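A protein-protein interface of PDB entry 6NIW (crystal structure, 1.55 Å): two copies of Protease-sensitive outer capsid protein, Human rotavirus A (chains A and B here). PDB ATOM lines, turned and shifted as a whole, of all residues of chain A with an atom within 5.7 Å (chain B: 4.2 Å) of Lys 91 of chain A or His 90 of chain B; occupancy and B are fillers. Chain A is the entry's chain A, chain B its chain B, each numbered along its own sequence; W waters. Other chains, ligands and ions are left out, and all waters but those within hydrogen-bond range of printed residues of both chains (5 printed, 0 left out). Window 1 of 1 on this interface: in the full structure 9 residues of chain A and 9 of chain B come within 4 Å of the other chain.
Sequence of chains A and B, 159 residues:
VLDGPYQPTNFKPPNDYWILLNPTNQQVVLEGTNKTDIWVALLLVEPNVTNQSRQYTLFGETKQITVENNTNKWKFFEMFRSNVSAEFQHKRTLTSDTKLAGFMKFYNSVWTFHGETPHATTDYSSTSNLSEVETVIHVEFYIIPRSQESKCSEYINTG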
ATOM      1  N   GLU A  78      11.950  18.494  -2.094  1.00  0.00           N
ATOM      2  CA  GLU A  78      13.010  17.511  -1.845  1.00  0.00           C
ATOM      3  C   GLU A  78      14.338  18.157  -2.290  1.00  0.00           C
ATOM      4  O   GLU A  78      14.555  18.337  -3.529  1.00  0.00           O
ATOM      5  CB  GLU A  78      12.701  16.162  -2.504  1.00  0.00           C
ATOM      6  CG  GLU A  78      13.833  15.196  -2.337  1.00  0.00           C
ATOM      7  CD  GLU A  78      13.605  13.832  -2.942  1.00  0.00           C
ATOM      8  OE1 GLU A  78      12.439  13.353  -2.891  1.00  0.00           O
ATOM      9  OE2 GLU A  78      14.591  13.286  -3.510  1.00  0.00           O
ATOM     10  N   MET A  79      15.115  18.619  -1.292  1.00  0.00           N
ATOM     11  CA  MET A  79      16.458  19.218  -1.470  1.00  0.00           C
ATOM     12  C   MET A  79      17.544  18.120  -1.400  1.00  0.00           C
ATOM     13  O   MET A  79      17.466  17.246  -0.557  1.00  0.00           O
ATOM     14  CB  MET A  79      16.721  20.289  -0.420  1.00  0.00           C
ATOM     15  CG  MET A  79      15.598  21.329  -0.346  1.00  0.00           C
ATOM     16  SD  MET A  79      15.166  22.154  -1.898  1.00  0.00           S
ATOM     17  CE  MET A  79      16.755  22.928  -2.267  1.00  0.00           C
ATOM     18  N   PHE A  80      18.508  18.160  -2.304  1.00  0.00           N
ATOM     19  CA  PHE A  80      19.452  17.027  -2.452  1.00  0.00           C
ATOM     20  C   PHE A  80      20.864  17.530  -2.726  1.00  0.00           C
ATOM     21  O   PHE A  80      21.012  18.544  -3.376  1.00  0.00           O
ATOM     22  CB  PHE A  80      19.001  16.164  -3.621  1.00  0.00           C
ATOM     23  CG  PHE A  80      19.878  14.960  -3.809  1.00  0.00           C
ATOM     24  CD1 PHE A  80      19.651  13.806  -3.077  1.00  0.00           C
ATOM     25  CD2 PHE A  80      20.930  15.002  -4.699  1.00  0.00           C
ATOM     26  CE1 PHE A  80      20.494  12.718  -3.222  1.00  0.00           C
ATOM     27  CE2 PHE A  80      21.767  13.899  -4.838  1.00  0.00           C
ATOM     28  CZ  PHE A  80      21.506  12.758  -4.132  1.00  0.00           C
ATOM     29  N   GLN A  89      20.353  21.229  -4.216  1.00  0.00           N
ATOM     30  CA  GLN A  89      19.510  21.438  -5.421  1.00  0.00           C
ATOM     31  C   GLN A  89      18.072  20.984  -5.090  1.00  0.00           C
ATOM     32  O   GLN A  89      17.877  20.103  -4.250  1.00  0.00           O
ATOM     33  CB  GLN A  89      20.093  20.656  -6.586  1.00  0.00           C
ATOM     34  CG  GLN A  89      19.713  19.204  -6.478  1.00  0.00           C
ATOM     35  CD  GLN A  89      20.719  18.175  -6.935  1.00  0.00           C
ATOM     36  OE1 GLN A  89      21.894  18.079  -6.437  1.00  0.00           O
ATOM     37  NE2 GLN A  89      20.123  17.205  -7.615  1.00  0.00           N
ATOM     38  N   HIS A  90      17.099  21.661  -5.669  1.00  0.00           N
ATOM     39  CA  HIS A  90      15.671  21.283  -5.599  1.00  0.00           C
ATOM     40  C   HIS A  90      15.428  20.166  -6.591  1.00  0.00           C
ATOM     41  O   HIS A  90      15.338  20.461  -7.803  1.00  0.00           O
ATOM     42  CB  HIS A  90      14.796  22.500  -5.815  1.00  0.00           C
ATOM     43  CG  HIS A  90      13.318  22.190  -5.775  1.00  0.00           C
ATOM     44  ND1 HIS A  90      12.374  23.049  -6.272  1.00  0.00           N
ATOM     45  CD2 HIS A  90      12.634  21.094  -5.366  1.00  0.00           C
ATOM     46  CE1 HIS A  90      11.157  22.564  -6.054  1.00  0.00           C
ATOM     47  NE2 HIS A  90      11.297  21.329  -5.583  1.00  0.00           N
ATOM     48  N   LYS A  91      15.450  18.948  -6.122  1.00  0.00           N
ATOM     49  CA  LYS A  91      15.490  17.762  -6.987  1.00  0.00           C
ATOM     50  C   LYS A  91      14.096  17.301  -7.390  1.00  0.00           C
ATOM     51  O   LYS A  91      13.885  16.982  -8.613  1.00  0.00           O
ATOM     52  CB  LYS A  91      16.274  16.669  -6.291  1.00  0.00           C
ATOM     53  CG  LYS A  91      16.585  15.497  -7.181  1.00  0.00           C
ATOM     54  CD  LYS A  91      17.377  14.455  -6.491  1.00  0.00           C
ATOM     55  CE  LYS A  91      17.615  13.275  -7.395  1.00  0.00           C
ATOM     56  NZ  LYS A  91      18.823  12.519  -6.978  1.00  0.00           N
ATOM     57  N   ARG A  92      13.141  17.331  -6.447  1.00  0.00           N
ATOM     58  CA  ARG A  92      11.758  16.854  -6.678  1.00  0.00           C
ATOM     59  C   ARG A  92      10.780  17.640  -5.829  1.00  0.00           C
ATOM     60  O   ARG A  92      11.210  18.330  -4.910  1.00  0.00           O
ATOM     61  CB  ARG A  92      11.618  15.375  -6.327  1.00  0.00           C
ATOM     62  CG  ARG A  92      12.459  14.505  -7.219  1.00  0.00           C
ATOM     63  CD  ARG A  92      12.200  13.039  -7.078  1.00  0.00           C
ATOM     64  NE  ARG A  92      13.143  12.507  -6.155  1.00  0.00           N
ATOM     65  CZ  ARG A  92      14.104  11.624  -6.410  1.00  0.00           C
ATOM     66  NH1 ARG A  92      14.377  11.193  -7.628  1.00  0.00           N
ATOM     67  NH2 ARG A  92      14.871  11.261  -5.406  1.00  0.00           N
ATOM     68  N   THR A  93       9.521  17.524  -6.174  1.00  0.00           N
ATOM     69  CA  THR A  93       8.420  18.108  -5.390  1.00  0.00           C
ATOM     70  C   THR A  93       7.285  17.090  -5.283  1.00  0.00           C
ATOM     71  O   THR A  93       6.868  16.490  -6.319  1.00  0.00           O
ATOM     72  CB  THR A  93       7.922  19.380  -6.008  1.00  0.00           C
ATOM     73  OG1 THR A  93       9.018  20.221  -6.377  1.00  0.00           O
ATOM     74  CG2 THR A  93       6.952  20.106  -5.098  1.00  0.00           C
ATOM     75  N   TYR A 124      14.001   7.343  -6.711  1.00  0.00           N
ATOM     76  CA  TYR A 124      15.141   6.999  -5.836  1.00  0.00           C
ATOM     77  C   TYR A 124      16.284   7.962  -6.088  1.00  0.00           C
ATOM     78  O   TYR A 124      16.392   8.560  -7.184  1.00  0.00           O
ATOM     79  CB  TYR A 124      15.536   5.528  -5.999  1.00  0.00           C
ATOM     80  CG  TYR A 124      16.066   5.144  -7.354  1.00  0.00           C
ATOM     81  CD1 TYR A 124      17.411   5.264  -7.679  1.00  0.00           C
ATOM     82  CD2 TYR A 124      15.210   4.631  -8.311  1.00  0.00           C
ATOM     83  CE1 TYR A 124      17.889   4.903  -8.930  1.00  0.00           C
ATOM     84  CE2 TYR A 124      15.680   4.239  -9.541  1.00  0.00           C
ATOM     85  CZ  TYR A 124      17.021   4.393  -9.856  1.00  0.00           C
ATOM     86  OH  TYR A 124      17.430   3.982 -11.089  1.00  0.00           O
ATOM     87  N   SER A 125      17.180   8.038  -5.115  1.00  0.00           N
ATOM     88  CA  SER A 125      18.558   8.525  -5.230  1.00  0.00           C
ATOM     89  C   SER A 125      19.515   7.387  -4.845  1.00  0.00           C
ATOM     90  O   SER A 125      19.252   6.673  -3.916  1.00  0.00           O
ATOM     91  CB  SER A 125      18.770   9.724  -4.406  1.00  0.00           C
ATOM     92  OG  SER A 125      17.806  10.736  -4.739  1.00  0.00           O
ATOM     93  N   GLU B  68      19.695  14.225 -13.327  1.00  0.00           N
ATOM     94  CA  GLU B  68      19.501  12.762 -13.187  1.00  0.00           C
ATOM     95  C   GLU B  68      18.209  12.429 -13.901  1.00  0.00           C
ATOM     96  O   GLU B  68      17.212  13.165 -13.764  1.00  0.00           O
ATOM     97  CB  GLU B  68      19.530  12.336 -11.715  1.00  0.00           C
ATOM     98  CG  GLU B  68      19.325  10.856 -11.475  1.00  0.00           C
ATOM     99  CD  GLU B  68      19.425  10.509  -9.992  1.00  0.00           C
ATOM    100  OE1 GLU B  68      18.449  10.865  -9.245  1.00  0.00           O
ATOM    101  OE2 GLU B  68      20.524  10.089  -9.557  1.00  0.00           O
ATOM    102  N   PHE B  77      13.821  19.729 -17.610  1.00  0.00           N
ATOM    103  CA  PHE B  77      14.164  20.444 -16.368  1.00  0.00           C
ATOM    104  C   PHE B  77      13.903  21.923 -16.582  1.00  0.00           C
ATOM    105  O   PHE B  77      14.348  22.498 -17.585  1.00  0.00           O
ATOM    106  CB  PHE B  77      15.648  20.283 -16.015  1.00  0.00           C
ATOM    107  CG  PHE B  77      16.009  19.025 -15.257  1.00  0.00           C
ATOM    108  CD1 PHE B  77      15.535  17.791 -15.626  1.00  0.00           C
ATOM    109  CD2 PHE B  77      16.854  19.100 -14.155  1.00  0.00           C
ATOM    110  CE1 PHE B  77      15.917  16.653 -14.923  1.00  0.00           C
ATOM    111  CE2 PHE B  77      17.200  17.975 -13.449  1.00  0.00           C
ATOM    112  CZ  PHE B  77      16.682  16.770 -13.787  1.00  0.00           C
ATOM    113  N   GLU B  78      12.968  22.464 -15.829  1.00  0.00           N
ATOM    114  CA  GLU B  78      12.652  23.891 -15.889  1.00  0.00           C
ATOM    115  C   GLU B  78      13.535  24.597 -14.875  1.00  0.00           C
ATOM    116  O   GLU B  78      13.331  24.416 -13.630  1.00  0.00           O
ATOM    117  CB  GLU B  78      11.187  24.143 -15.635  1.00  0.00           C
ATOM    118  CG  GLU B  78      10.857  25.615 -15.590  1.00  0.00           C
ATOM    119  CD  GLU B  78       9.393  25.906 -15.404  1.00  0.00           C
ATOM    120  OE1 GLU B  78       8.544  25.058 -15.850  1.00  0.00           O
ATOM    121  OE2 GLU B  78       9.095  26.965 -14.809  1.00  0.00           O
ATOM    122  N   MET B  79      14.409  25.439 -15.390  1.00  0.00           N
ATOM    123  CA  MET B  79      15.412  26.198 -14.596  1.00  0.00           C
ATOM    124  C   MET B  79      14.924  27.630 -14.557  1.00  0.00           C
ATOM    125  O   MET B  79      14.462  28.106 -15.577  1.00  0.00           O
ATOM    126  CB  MET B  79      16.790  26.164 -15.259  1.00  0.00           C
ATOM    127  CG  MET B  79      17.339  24.773 -15.504  1.00  0.00           C
ATOM    128  SD  MET B  79      17.324  23.629 -14.111  1.00  0.00           S
ATOM    129  CE  MET B  79      18.432  24.431 -12.942  1.00  0.00           C
ATOM    130  N   GLN B  89      17.553  28.038 -10.201  1.00  0.00           N
ATOM    131  CA  GLN B  89      16.981  26.943  -9.381  1.00  0.00           C
ATOM    132  C   GLN B  89      16.293  25.942 -10.299  1.00  0.00           C
ATOM    133  O   GLN B  89      15.873  26.330 -11.385  1.00  0.00           O
ATOM    134  CB  GLN B  89      16.085  27.549  -8.299  1.00  0.00           C
ATOM    135  CG  GLN B  89      14.869  28.228  -8.865  1.00  0.00           C
ATOM    136  CD  GLN B  89      14.332  29.404  -8.070  1.00  0.00           C
ATOM    137  OE1 GLN B  89      14.853  30.535  -8.132  1.00  0.00           O
ATOM    138  NE2 GLN B  89      13.100  29.241  -7.655  1.00  0.00           N
ATOM    139  N   HIS B  90      16.330  24.660  -9.961  1.00  0.00           N
ATOM    140  CA  HIS B  90      15.525  23.625 -10.655  1.00  0.00           C
ATOM    141  C   HIS B  90      14.088  23.702 -10.125  1.00  0.00           C
ATOM    142  O   HIS B  90      13.841  23.190  -9.009  1.00  0.00           O
ATOM    143  CB  HIS B  90      16.149  22.283 -10.492  1.00  0.00           C
ATOM    144  CG  HIS B  90      15.346  21.218 -11.105  1.00  0.00           C
ATOM    145  ND1 HIS B  90      15.565  19.894 -10.789  1.00  0.00           N
ATOM    146  CD2 HIS B  90      14.417  21.236 -12.092  1.00  0.00           C
ATOM    147  CE1 HIS B  90      14.756  19.137 -11.485  1.00  0.00           C
ATOM    148  NE2 HIS B  90      14.017  19.932 -12.299  1.00  0.00           N
ATOM    149  N   LYS B  91      13.231  24.427 -10.853  1.00  0.00           N
ATOM    150  CA  LYS B  91      11.898  24.839 -10.329  1.00  0.00           C
ATOM    151  C   LYS B  91      10.912  23.686 -10.542  1.00  0.00           C
ATOM    152  O   LYS B  91      10.173  23.374  -9.599  1.00  0.00           O
ATOM    153  CB  LYS B  91      11.509  26.146 -10.938  1.00  0.00           C
ATOM    154  CG  LYS B  91      10.210  26.675 -10.394  1.00  0.00           C
ATOM    155  CD  LYS B  91      10.074  28.117 -10.608  1.00  0.00           C
ATOM    156  CE  LYS B  91       8.791  28.662 -10.050  1.00  0.00           C
ATOM    157  NZ  LYS B  91       8.835  30.142  -9.991  1.00  0.00           N
ATOM    158  N   ARG B  92      10.891  23.088 -11.723  1.00  0.00           N
ATOM    159  CA  ARG B  92       9.893  22.058 -12.099  1.00  0.00           C
ATOM    160  C   ARG B  92      10.479  21.034 -13.021  1.00  0.00           C
ATOM    161  O   ARG B  92      11.594  21.241 -13.542  1.00  0.00           O
ATOM    162  CB  ARG B  92       8.694  22.726 -12.753  1.00  0.00           C
ATOM    163  CG  ARG B  92       8.000  23.672 -11.803  1.00  0.00           C
ATOM    164  CD  ARG B  92       6.648  24.147 -12.290  1.00  0.00           C
ATOM    165  NE  ARG B  92       6.847  25.389 -12.937  1.00  0.00           N
ATOM    166  CZ  ARG B  92       6.463  26.586 -12.509  1.00  0.00           C
ATOM    167  NH1 ARG B  92       5.803  26.786 -11.373  1.00  0.00           N
ATOM    168  NH2 ARG B  92       6.793  27.612 -13.236  1.00  0.00           N
ATOM    169  N   THR B  93       9.775  19.942 -13.175  1.00  0.00           N
ATOM    170  CA  THR B  93      10.190  18.876 -14.081  1.00  0.00           C
ATOM    171  C   THR B  93       8.956  18.435 -14.844  1.00  0.00           C
ATOM    172  O   THR B  93       7.883  18.293 -14.186  1.00  0.00           O
ATOM    173  CB  THR B  93      10.878  17.730 -13.369  1.00  0.00           C
ATOM    174  OG1 THR B  93      11.905  18.282 -12.534  1.00  0.00           O
ATOM    175  CG2 THR B  93      11.436  16.758 -14.379  1.00  0.00           C
HETATM  176  O   HOH W   1      16.112  11.556 -10.186  1.00  0.00           O
HETATM  177  O   HOH W   2      12.701  20.674  -8.919  1.00  0.00           O
HETATM  178  O   HOH W   3      17.999  18.623  -9.432  1.00  0.00           O
HETATM  179  O   HOH W   4      12.716  25.940  -6.934  1.00  0.00           O
HETATM  180  O   HOH W   5      18.034  24.037  -7.428  1.00  0.00           O
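O of His 90 of chain A sits at hydrogen-bond distance from ND1 of His 90 of chain B.
The side-chain amino group (NZ) of Lys 91 of chain A lies within salt-bridge range of the side-chain carboxylate (OE1) of Glu 68 of chain B (2.8 Å).
A ring nitrogen (NE2) of His 90 of chain A sits at hydrogen-bond distance from the backbone carbonyl oxygen (O) of Arg 92 of chain A.
OG of Ser 125 of chain A is in hydrogen-bond range of NZ of Lys 91 of chain A.
The backbone NH (N) of Lys 91 of chain B sits at hydrogen-bond distance from the backbone carbonyl oxygen (O) of Glu 78 of chain B (2.8 Å).
The backbone carbonyl oxygen (O) of Arg 92 of chain B lies within hydrogen-bond range of a ring nitrogen (NE2) of His 90 of chain B (3.0 Å).
A ring nitrogen (NE2) of His 90 of chain A sits at hydrogen-bond distance from the side-chain hydroxyl (OG1) of Thr 93 of chain A (2.7 Å).
A ring nitrogen (NE2) of His 90 of chain B is in hydrogen-bond range of the side-chain hydroxyl (OG1) of Thr 93 of chain B (2.7 Å).
Among the printed residues, pairs that only touch across the chains: Lys 91 of chain A with His 90 of chain B (3.7 Å), Tyr 124 of chain A with Glu 68 of chain B (3.7 Å) and His 90 of chain A with Lys 91 of chain B (3.8 Å).
Glu 78 of chain A touches none of the printed residues of chain B.
Of the printed residues of chain B, His 90 of chain A touches His 90 (3.0 Å) and Lys 91 (3.8 Å).
Lys 91 of chain A touches just these residues of chain B: Glu 68 and His 90.
Of the printed residues of chain A, Glu 68 of chain B touches Lys 91 and Tyr 124.
Of the printed residues of chain A, Lys 91 of chain B touches His 90 (3.8 Å).
Arg 92 of chain B touches none of the printed residues of chain A.
The nearest printed residue of chain B that does not touch Lys 91 of chain A is Thr 93 of chain B (4.6 Å).
The nearest residue of chain A that does not touch His 90 of chain B is Arg 92 of chain A (5.6 Å).
Of the 10 printed residues of chain A, 3 touch a printed residue of chain B.
Hydrophobic or aromatic side chains of chain A that line the printed part of chain B: His 90.
Printed residues of chain B that touch a printed residue of chain A: Glu 68, His 90 and Lys 91.
Hydrophobic or aromatic side chains of chain B within 4 Å of the printed part of chain A: His 90.
Among the printed residues, 5 pairs touch across the chains.
Among the printed residues, Asp or Glu carboxylates within 4 Å of a Lys or Arg side-chain nitrogen of the other chain: Lys 91 of chain A with Glu 68 of chain B (2.8 Å).
His 90 of chain A touches its own counterpart, His 90 of chain B.
His 90 of chain A touches Lys 91 of chain B, and with the chains exchanged Lys 91 of chain A touches His 90 of chain B.
Of the 5 pairs that touch across the chains among the printed residues, 3 have their exchanged pair printed and touching as well.
Water W1 bridges the side-chain carboxylate (OE1) of Glu 68 of chain B (2.6 Å) and the guanidinium group (NH1) of Arg 92 of chain A (3.1 Å).
Water W2 bridges O of His 90 of chain B and O of His 90 of chain A.
Water W4 bridges a ring nitrogen (ND1) of His 90 of chain A (3.0 Å) and the side-chain amide nitrogen of Gln 89 of chain B (3.4 Å).
Water W3 lies within hydrogen-bond range of ND1 of His 90 of chain B (3.1 Å) and NE2 of Gln 89 of chain A (3.1 Å).
Water W5 lies within hydrogen-bond range of N of His 90 of chain A (3.1 Å) and N of His 90 of chain B (3.1 Å).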
